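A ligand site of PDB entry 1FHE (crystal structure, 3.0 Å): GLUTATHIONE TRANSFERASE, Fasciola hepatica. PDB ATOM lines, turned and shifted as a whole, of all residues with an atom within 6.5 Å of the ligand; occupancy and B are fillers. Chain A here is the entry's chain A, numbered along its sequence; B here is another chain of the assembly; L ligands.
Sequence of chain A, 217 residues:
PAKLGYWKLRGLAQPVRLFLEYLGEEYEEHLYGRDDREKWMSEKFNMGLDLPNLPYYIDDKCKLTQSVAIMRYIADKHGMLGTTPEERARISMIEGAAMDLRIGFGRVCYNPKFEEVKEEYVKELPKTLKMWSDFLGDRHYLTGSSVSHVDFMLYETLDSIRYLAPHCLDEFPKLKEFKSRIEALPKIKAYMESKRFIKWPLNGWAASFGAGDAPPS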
ATOM      1  N   TYR A   6      10.430  -2.225  -3.527  1.00  0.00           N
ATOM      2  CA  TYR A   6      10.180  -1.835  -4.905  1.00  0.00           C
ATOM      3  C   TYR A   6       8.874  -2.494  -5.319  1.00  0.00           C
ATOM      4  O   TYR A   6       8.445  -3.474  -4.708  1.00  0.00           O
ATOM      5  CB  TYR A   6      11.294  -2.329  -5.817  1.00  0.00           C
ATOM      6  CG  TYR A   6      11.621  -1.427  -6.986  1.00  0.00           C
ATOM      7  CD1 TYR A   6      12.506  -0.353  -6.831  1.00  0.00           C
ATOM      8  CD2 TYR A   6      11.094  -1.669  -8.250  1.00  0.00           C
ATOM      9  CE1 TYR A   6      12.869   0.435  -7.914  1.00  0.00           C
ATOM     10  CE2 TYR A   6      11.452  -0.873  -9.334  1.00  0.00           C
ATOM     11  CZ  TYR A   6      12.343   0.170  -9.159  1.00  0.00           C
ATOM     12  OH  TYR A   6      12.738   0.944 -10.229  1.00  0.00           O
ATOM     13  N   TRP A   7       8.245  -1.964  -6.360  1.00  0.00           N
ATOM     14  CA  TRP A   7       7.000  -2.539  -6.849  1.00  0.00           C
ATOM     15  C   TRP A   7       7.346  -3.686  -7.783  1.00  0.00           C
ATOM     16  O   TRP A   7       8.474  -3.762  -8.273  1.00  0.00           O
ATOM     17  CB  TRP A   7       6.152  -1.525  -7.614  1.00  0.00           C
ATOM     18  CG  TRP A   7       6.620  -0.108  -7.549  1.00  0.00           C
ATOM     19  CD1 TRP A   7       7.797   0.401  -8.032  1.00  0.00           C
ATOM     20  CD2 TRP A   7       5.877   1.014  -7.058  1.00  0.00           C
ATOM     21  NE1 TRP A   7       7.825   1.762  -7.855  1.00  0.00           N
ATOM     22  CE2 TRP A   7       6.664   2.170  -7.265  1.00  0.00           C
ATOM     23  CE3 TRP A   7       4.620   1.143  -6.453  1.00  0.00           C
ATOM     24  CZ2 TRP A   7       6.228   3.440  -6.891  1.00  0.00           C
ATOM     25  CZ3 TRP A   7       4.184   2.414  -6.079  1.00  0.00           C
ATOM     26  CH2 TRP A   7       4.991   3.546  -6.299  1.00  0.00           C
ATOM     27  N   LEU A  12      14.887  -0.898 -11.204  1.00  0.00           N
ATOM     28  CA  LEU A  12      16.307  -0.830 -10.902  1.00  0.00           C
ATOM     29  C   LEU A  12      16.577  -1.709  -9.698  1.00  0.00           C
ATOM     30  O   LEU A  12      17.580  -1.544  -8.997  1.00  0.00           O
ATOM     31  CB  LEU A  12      16.723   0.615 -10.585  1.00  0.00           C
ATOM     32  CG  LEU A  12      16.553   1.675 -11.673  1.00  0.00           C
ATOM     33  CD1 LEU A  12      17.428   2.872 -11.336  1.00  0.00           C
ATOM     34  CD2 LEU A  12      16.916   1.114 -13.034  1.00  0.00           C
ATOM     35  N   ARG A  37       0.564   3.281  -4.955  1.00  0.00           N
ATOM     36  CA  ARG A  37       1.550   4.358  -5.054  1.00  0.00           C
ATOM     37  C   ARG A  37       1.310   5.151  -3.785  1.00  0.00           C
ATOM     38  O   ARG A  37       2.243   5.671  -3.165  1.00  0.00           O
ATOM     39  CB  ARG A  37       1.313   5.270  -6.263  1.00  0.00           C
ATOM     40  CG  ARG A  37       1.779   6.710  -5.994  1.00  0.00           C
ATOM     41  CD  ARG A  37       2.506   7.324  -7.180  1.00  0.00           C
ATOM     42  NE  ARG A  37       3.956   7.431  -6.955  1.00  0.00           N
ATOM     43  CZ  ARG A  37       4.656   8.543  -7.149  1.00  0.00           C
ATOM     44  NH1 ARG A  37       4.053   9.643  -7.572  1.00  0.00           N
ATOM     45  NH2 ARG A  37       5.965   8.543  -6.941  1.00  0.00           N
ATOM     46  N   TRP A  40       2.147   3.470  -0.762  1.00  0.00           N
ATOM     47  CA  TRP A  40       3.562   3.672  -0.580  1.00  0.00           C
ATOM     48  C   TRP A  40       3.793   5.102  -0.094  1.00  0.00           C
ATOM     49  O   TRP A  40       4.440   5.314   0.933  1.00  0.00           O
ATOM     50  CB  TRP A  40       4.309   3.428  -1.891  1.00  0.00           C
ATOM     51  CG  TRP A  40       5.627   4.103  -1.952  1.00  0.00           C
ATOM     52  CD1 TRP A  40       6.110   4.878  -2.960  1.00  0.00           C
ATOM     53  CD2 TRP A  40       6.646   4.080  -0.938  1.00  0.00           C
ATOM     54  NE1 TRP A  40       7.364   5.342  -2.646  1.00  0.00           N
ATOM     55  CE2 TRP A  40       7.717   4.869  -1.405  1.00  0.00           C
ATOM     56  CE3 TRP A  40       6.743   3.475   0.317  1.00  0.00           C
ATOM     57  CZ2 TRP A  40       8.884   5.071  -0.659  1.00  0.00           C
ATOM     58  CZ3 TRP A  40       7.915   3.669   1.063  1.00  0.00           C
ATOM     59  CH2 TRP A  40       8.962   4.464   0.570  1.00  0.00           C
ATOM     60  N   MET A  41       3.259   6.060  -0.840  1.00  0.00           N
ATOM     61  CA  MET A  41       3.388   7.485  -0.514  1.00  0.00           C
ATOM     62  C   MET A  41       3.400   7.762   0.984  1.00  0.00           C
ATOM     63  O   MET A  41       4.391   8.268   1.521  1.00  0.00           O
ATOM     64  CB  MET A  41       2.234   8.269  -1.153  1.00  0.00           C
ATOM     65  CG  MET A  41       2.448   8.624  -2.609  1.00  0.00           C
ATOM     66  SD  MET A  41       4.185   8.823  -3.026  1.00  0.00           S
ATOM     67  CE  MET A  41       4.525  10.402  -2.250  1.00  0.00           C
ATOM     68  N   LYS A  44       6.478   6.469   2.575  1.00  0.00           N
ATOM     69  CA  LYS A  44       7.741   7.035   2.087  1.00  0.00           C
ATOM     70  C   LYS A  44       8.598   7.736   3.148  1.00  0.00           C
ATOM     71  O   LYS A  44       9.823   7.827   2.983  1.00  0.00           O
ATOM     72  CB  LYS A  44       7.465   7.996   0.925  1.00  0.00           C
ATOM     73  CG  LYS A  44       8.555   9.038   0.693  1.00  0.00           C
ATOM     74  CD  LYS A  44       9.130   8.952  -0.700  1.00  0.00           C
ATOM     75  CE  LYS A  44      10.218   9.995  -0.896  1.00  0.00           C
ATOM     76  NZ  LYS A  44      10.546  10.187  -2.334  1.00  0.00           N
ATOM     77  N   PRO A  52      14.824   9.460   1.302  1.00  0.00           N
ATOM     78  CA  PRO A  52      13.813   8.502   0.868  1.00  0.00           C
ATOM     79  C   PRO A  52      13.839   8.204  -0.616  1.00  0.00           C
ATOM     80  O   PRO A  52      14.274   9.032  -1.420  1.00  0.00           O
ATOM     81  CB  PRO A  52      12.497   9.135   1.306  1.00  0.00           C
ATOM     82  CG  PRO A  52      12.877   9.971   2.472  1.00  0.00           C
ATOM     83  CD  PRO A  52      14.231  10.522   2.133  1.00  0.00           C
ATOM     84  N   ASN A  53      13.382   7.004  -0.973  1.00  0.00           N
ATOM     85  CA  ASN A  53      13.336   6.568  -2.368  1.00  0.00           C
ATOM     86  C   ASN A  53      13.095   5.058  -2.486  1.00  0.00           C
ATOM     87  O   ASN A  53      12.792   4.400  -1.495  1.00  0.00           O
ATOM     88  CB  ASN A  53      14.649   6.926  -3.073  1.00  0.00           C
ATOM     89  CG  ASN A  53      14.561   6.790  -4.576  1.00  0.00           C
ATOM     90  OD1 ASN A  53      13.872   7.556  -5.240  1.00  0.00           O
ATOM     91  ND2 ASN A  53      15.260   5.792  -5.117  1.00  0.00           N
ATOM     92  N   LEU A  54      13.236   4.550  -3.709  1.00  0.00           N
ATOM     93  CA  LEU A  54      13.071   3.128  -4.007  1.00  0.00           C
ATOM     94  C   LEU A  54      14.067   2.749  -5.094  1.00  0.00           C
ATOM     95  O   LEU A  54      14.311   3.515  -6.038  1.00  0.00           O
ATOM     96  CB  LEU A  54      11.633   2.857  -4.482  1.00  0.00           C
ATOM     97  CG  LEU A  54      10.699   2.054  -3.581  1.00  0.00           C
ATOM     98  CD1 LEU A  54      10.674   2.648  -2.188  1.00  0.00           C
ATOM     99  CD2 LEU A  54       9.292   2.062  -4.157  1.00  0.00           C
ATOM    100  N   PRO A  55      14.667   1.543  -5.007  1.00  0.00           N
ATOM    101  CA  PRO A  55      14.450   0.550  -3.953  1.00  0.00           C
ATOM    102  C   PRO A  55      15.177   0.902  -2.665  1.00  0.00           C
ATOM    103  O   PRO A  55      16.310   1.373  -2.696  1.00  0.00           O
ATOM    104  CB  PRO A  55      14.998  -0.733  -4.579  1.00  0.00           C
ATOM    105  CG  PRO A  55      16.070  -0.259  -5.493  1.00  0.00           C
ATOM    106  CD  PRO A  55      15.680   1.110  -5.986  1.00  0.00           C
ATOM    107  N   THR A  65      19.426   3.621   0.704  1.00  0.00           N
ATOM    108  CA  THR A  65      18.534   3.889  -0.423  1.00  0.00           C
ATOM    109  C   THR A  65      19.430   4.194  -1.620  1.00  0.00           C
ATOM    110  O   THR A  65      20.518   4.731  -1.452  1.00  0.00           O
ATOM    111  CB  THR A  65      17.626   5.094  -0.141  1.00  0.00           C
ATOM    112  OG1 THR A  65      18.402   6.166   0.389  1.00  0.00           O
ATOM    113  CG2 THR A  65      16.535   4.720   0.850  1.00  0.00           C
ATOM    114  N   GLN A  66      18.944   3.862  -2.811  1.00  0.00           N
ATOM    115  CA  GLN A  66      19.655   4.041  -4.080  1.00  0.00           C
ATOM    116  C   GLN A  66      20.128   2.669  -4.564  1.00  0.00           C
ATOM    117  O   GLN A  66      21.053   2.089  -4.007  1.00  0.00           O
ATOM    118  CB  GLN A  66      20.879   4.967  -3.931  1.00  0.00           C
ATOM    119  CG  GLN A  66      20.546   6.432  -3.649  1.00  0.00           C
ATOM    120  CD  GLN A  66      20.388   7.236  -4.915  1.00  0.00           C
ATOM    121  OE1 GLN A  66      20.950   6.898  -5.955  1.00  0.00           O
ATOM    122  NE2 GLN A  66      19.617   8.316  -4.832  1.00  0.00           N
ATOM    123  N   SER A  67      19.468   2.147  -5.604  1.00  0.00           N
ATOM    124  CA  SER A  67      19.799   0.845  -6.163  1.00  0.00           C
ATOM    125  C   SER A  67      21.286   0.529  -6.015  1.00  0.00           C
ATOM    126  O   SER A  67      21.653  -0.491  -5.433  1.00  0.00           O
ATOM    127  CB  SER A  67      19.421   0.795  -7.648  1.00  0.00           C
ATOM    128  OG  SER A  67      20.004   1.883  -8.355  1.00  0.00           O
ATOM    129  N   VAL A  68      22.119   1.408  -6.541  1.00  0.00           N
ATOM    130  CA  VAL A  68      23.564   1.238  -6.477  1.00  0.00           C
ATOM    131  C   VAL A  68      24.082   1.281  -5.035  1.00  0.00           C
ATOM    132  O   VAL A  68      24.821   0.403  -4.601  1.00  0.00           O
ATOM    133  CB  VAL A  68      24.294   2.320  -7.291  1.00  0.00           C
ATOM    134  CG1 VAL A  68      24.723   1.744  -8.632  1.00  0.00           C
ATOM    135  CG2 VAL A  68      23.383   3.518  -7.503  1.00  0.00           C
ATOM    136  N   ALA A  69      23.697   2.319  -4.299  1.00  0.00           N
ATOM    137  CA  ALA A  69      24.130   2.422  -2.921  1.00  0.00           C
ATOM    138  C   ALA A  69      23.649   1.177  -2.169  1.00  0.00           C
ATOM    139  O   ALA A  69      24.297   0.713  -1.234  1.00  0.00           O
ATOM    140  CB  ALA A  69      23.550   3.673  -2.289  1.00  0.00           C
ATOM    141  N   MET A  99      24.773   2.889 -15.804  1.00  0.00           N
ATOM    142  CA  MET A  99      23.614   3.721 -15.570  1.00  0.00           C
ATOM    143  C   MET A  99      23.467   4.645 -16.759  1.00  0.00           C
ATOM    144  O   MET A  99      22.359   5.070 -17.092  1.00  0.00           O
ATOM    145  CB  MET A  99      23.777   4.541 -14.278  1.00  0.00           C
ATOM    146  CG  MET A  99      22.747   4.212 -13.205  1.00  0.00           C
ATOM    147  SD  MET A  99      21.341   3.282 -13.830  1.00  0.00           S
ATOM    148  CE  MET A  99      20.771   2.478 -12.328  1.00  0.00           C
ATOM    149  N   ILE A 103      19.815   4.967 -17.812  1.00  0.00           N
ATOM    150  CA  ILE A 103      19.390   6.343 -17.580  1.00  0.00           C
ATOM    151  C   ILE A 103      19.015   6.989 -18.913  1.00  0.00           C
ATOM    152  O   ILE A 103      17.918   7.502 -19.084  1.00  0.00           O
ATOM    153  CB  ILE A 103      20.501   7.179 -16.888  1.00  0.00           C
ATOM    154  CG1 ILE A 103      20.296   7.169 -15.359  1.00  0.00           C
ATOM    155  CG2 ILE A 103      20.481   8.612 -17.391  1.00  0.00           C
ATOM    156  CD1 ILE A 103      18.865   7.019 -14.901  1.00  0.00           C
ATOM    157  N   TYR A 110       8.793   5.631 -20.192  1.00  0.00           N
ATOM    158  CA  TYR A 110       7.464   5.831 -19.626  1.00  0.00           C
ATOM    159  C   TYR A 110       6.647   6.890 -20.389  1.00  0.00           C
ATOM    160  O   TYR A 110       5.413   6.920 -20.302  1.00  0.00           O
ATOM    161  CB  TYR A 110       7.573   6.243 -18.147  1.00  0.00           C
ATOM    162  CG  TYR A 110       8.424   5.333 -17.270  1.00  0.00           C
ATOM    163  CD1 TYR A 110       9.819   5.375 -17.324  1.00  0.00           C
ATOM    164  CD2 TYR A 110       7.831   4.492 -16.335  1.00  0.00           C
ATOM    165  CE1 TYR A 110      10.603   4.612 -16.471  1.00  0.00           C
ATOM    166  CE2 TYR A 110       8.607   3.712 -15.471  1.00  0.00           C
ATOM    167  CZ  TYR A 110       9.987   3.780 -15.540  1.00  0.00           C
ATOM    168  OH  TYR A 110      10.760   3.045 -14.680  1.00  0.00           O
ATOM    169  N   ASN A 203       9.944  -2.204 -16.615  1.00  0.00           N
ATOM    170  CA  ASN A 203      10.070  -0.760 -16.520  1.00  0.00           C
ATOM    171  C   ASN A 203       8.959  -0.159 -15.664  1.00  0.00           C
ATOM    172  O   ASN A 203       9.137   0.884 -15.047  1.00  0.00           O
ATOM    173  CB  ASN A 203      10.046  -0.138 -17.925  1.00  0.00           C
ATOM    174  CG  ASN A 203      11.342  -0.346 -18.673  1.00  0.00           C
ATOM    175  OD1 ASN A 203      12.397  -0.573 -18.059  1.00  0.00           O
ATOM    176  ND2 ASN A 203      11.287  -0.269 -19.992  1.00  0.00           N
ATOM    177  N   GLY B  96      24.167   9.684  -4.927  1.00  0.00           N
ATOM    178  CA  GLY B  96      23.072   9.051  -5.634  1.00  0.00           C
ATOM    179  C   GLY B  96      21.981  10.083  -5.834  1.00  0.00           C
ATOM    180  O   GLY B  96      21.423  10.202  -6.916  1.00  0.00           O
ATOM    181  N   ASP B 100      20.618  12.349  -8.892  1.00  0.00           N
ATOM    182  CA  ASP B 100      19.167  12.234  -9.031  1.00  0.00           C
ATOM    183  C   ASP B 100      18.652  13.594  -9.494  1.00  0.00           C
ATOM    184  O   ASP B 100      17.746  13.690 -10.333  1.00  0.00           O
ATOM    185  CB  ASP B 100      18.522  11.875  -7.690  1.00  0.00           C
ATOM    186  CG  ASP B 100      18.195  10.395  -7.563  1.00  0.00           C
ATOM    187  OD1 ASP B 100      19.045   9.565  -7.949  1.00  0.00           O
ATOM    188  OD2 ASP B 100      17.094  10.068  -7.071  1.00  0.00           O
HETATM  189  N1  LIG L   1      18.547   6.856  -9.651  1.00  0.00           N
HETATM  190  C1  LIG L   1      17.502   6.282  -8.688  1.00  0.00           C
HETATM  191  C2  LIG L   1      18.140   5.436  -7.599  1.00  0.00           C
HETATM  192  O1  LIG L   1      19.358   5.322  -7.514  1.00  0.00           O
HETATM  193  O2  LIG L   1      17.326   4.816  -6.758  1.00  0.00           O
HETATM  194  C3  LIG L   1      16.810   7.466  -7.926  1.00  0.00           C
HETATM  195  C4  LIG L   1      15.448   7.067  -7.584  1.00  0.00           C
HETATM  196  C5  LIG L   1      14.300   7.013  -8.444  1.00  0.00           C
HETATM  197  O3  LIG L   1      14.206   7.993  -9.290  1.00  0.00           O
HETATM  198  N2  LIG L   1      13.305   6.212  -8.034  1.00  0.00           N
HETATM  199  C6  LIG L   1      12.167   5.762  -8.815  1.00  0.00           C
HETATM  200  C7  LIG L   1      10.944   5.574  -7.867  1.00  0.00           C
HETATM  201  O4  LIG L   1      10.198   4.548  -8.169  1.00  0.00           O
HETATM  202  C8  LIG L   1      12.411   4.662  -9.847  1.00  0.00           C
HETATM  203  S1  LIG L   1      12.388   5.184 -11.522  1.00  0.00           S
HETATM  204  N3  LIG L   1      10.453   6.718  -7.392  1.00  0.00           N
HETATM  205  C9  LIG L   1       9.455   6.890  -6.329  1.00  0.00           C
HETATM  206  C10 LIG L   1       9.475   8.203  -5.643  1.00  0.00           C
HETATM  207  O5  LIG L   1       9.589   9.347  -6.243  1.00  0.00           O
HETATM  208  O6  LIG L   1       9.131   8.295  -4.309  1.00  0.00           O
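The side-chain carboxylate of Asp 100 of chain B lies within hydrogen-bond range of the side-chain amide nitrogen of Gln 66 (3.4 Å). NE2 of Gln 66 sits close to O of Gly 96 of chain B (3.3 Å). O of Gly 96 of chain B sits close to OD1 of Asp 100 of chain B. The side-chain hydroxyl of Tyr 6 sits at hydrogen-bond distance from the backbone NH of Leu 12 (3.0 Å).
The side-chain amide oxygen (OE1) of Gln 66 sits close to an oxygen (O1) of the ligand (2.7 Å). A nitrogen (N1) of the ligand is in salt-bridge range of the side-chain carboxylate (OD1) of Asp 100 of chain B (3.2 Å). O2 of the ligand sits close to ND2 of Asn 53 (2.8 Å). NZ of Lys 44 lies within salt-bridge range of O6 of the ligand (3.1 Å). O5 of the ligand lies within salt-bridge range of NH2 of Arg 37 (3.8 Å).
An oxygen (O2) of the ligand sits close to the backbone carbonyl oxygen (O) of Leu 54 (3.4 Å). OH of Tyr 6 touches C8 of the ligand, 3.8 Å away. Trp 7 touches the ligand (NE1 to O4, 3.7 Å). Trp 40 touches the ligand. OG of Ser 67 touches O1 of the ligand (3.6 Å). Ten residues have an atom within 4 Å of the ligand: Tyr 6, Trp 7, Arg 37, Trp 40, Lys 44, Asn 53, Leu 54, Gln 66, Ser 67 and Asp 100 of chain B. Along chain A the residues within 4 Å of the ligand span positions 6 to 67.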
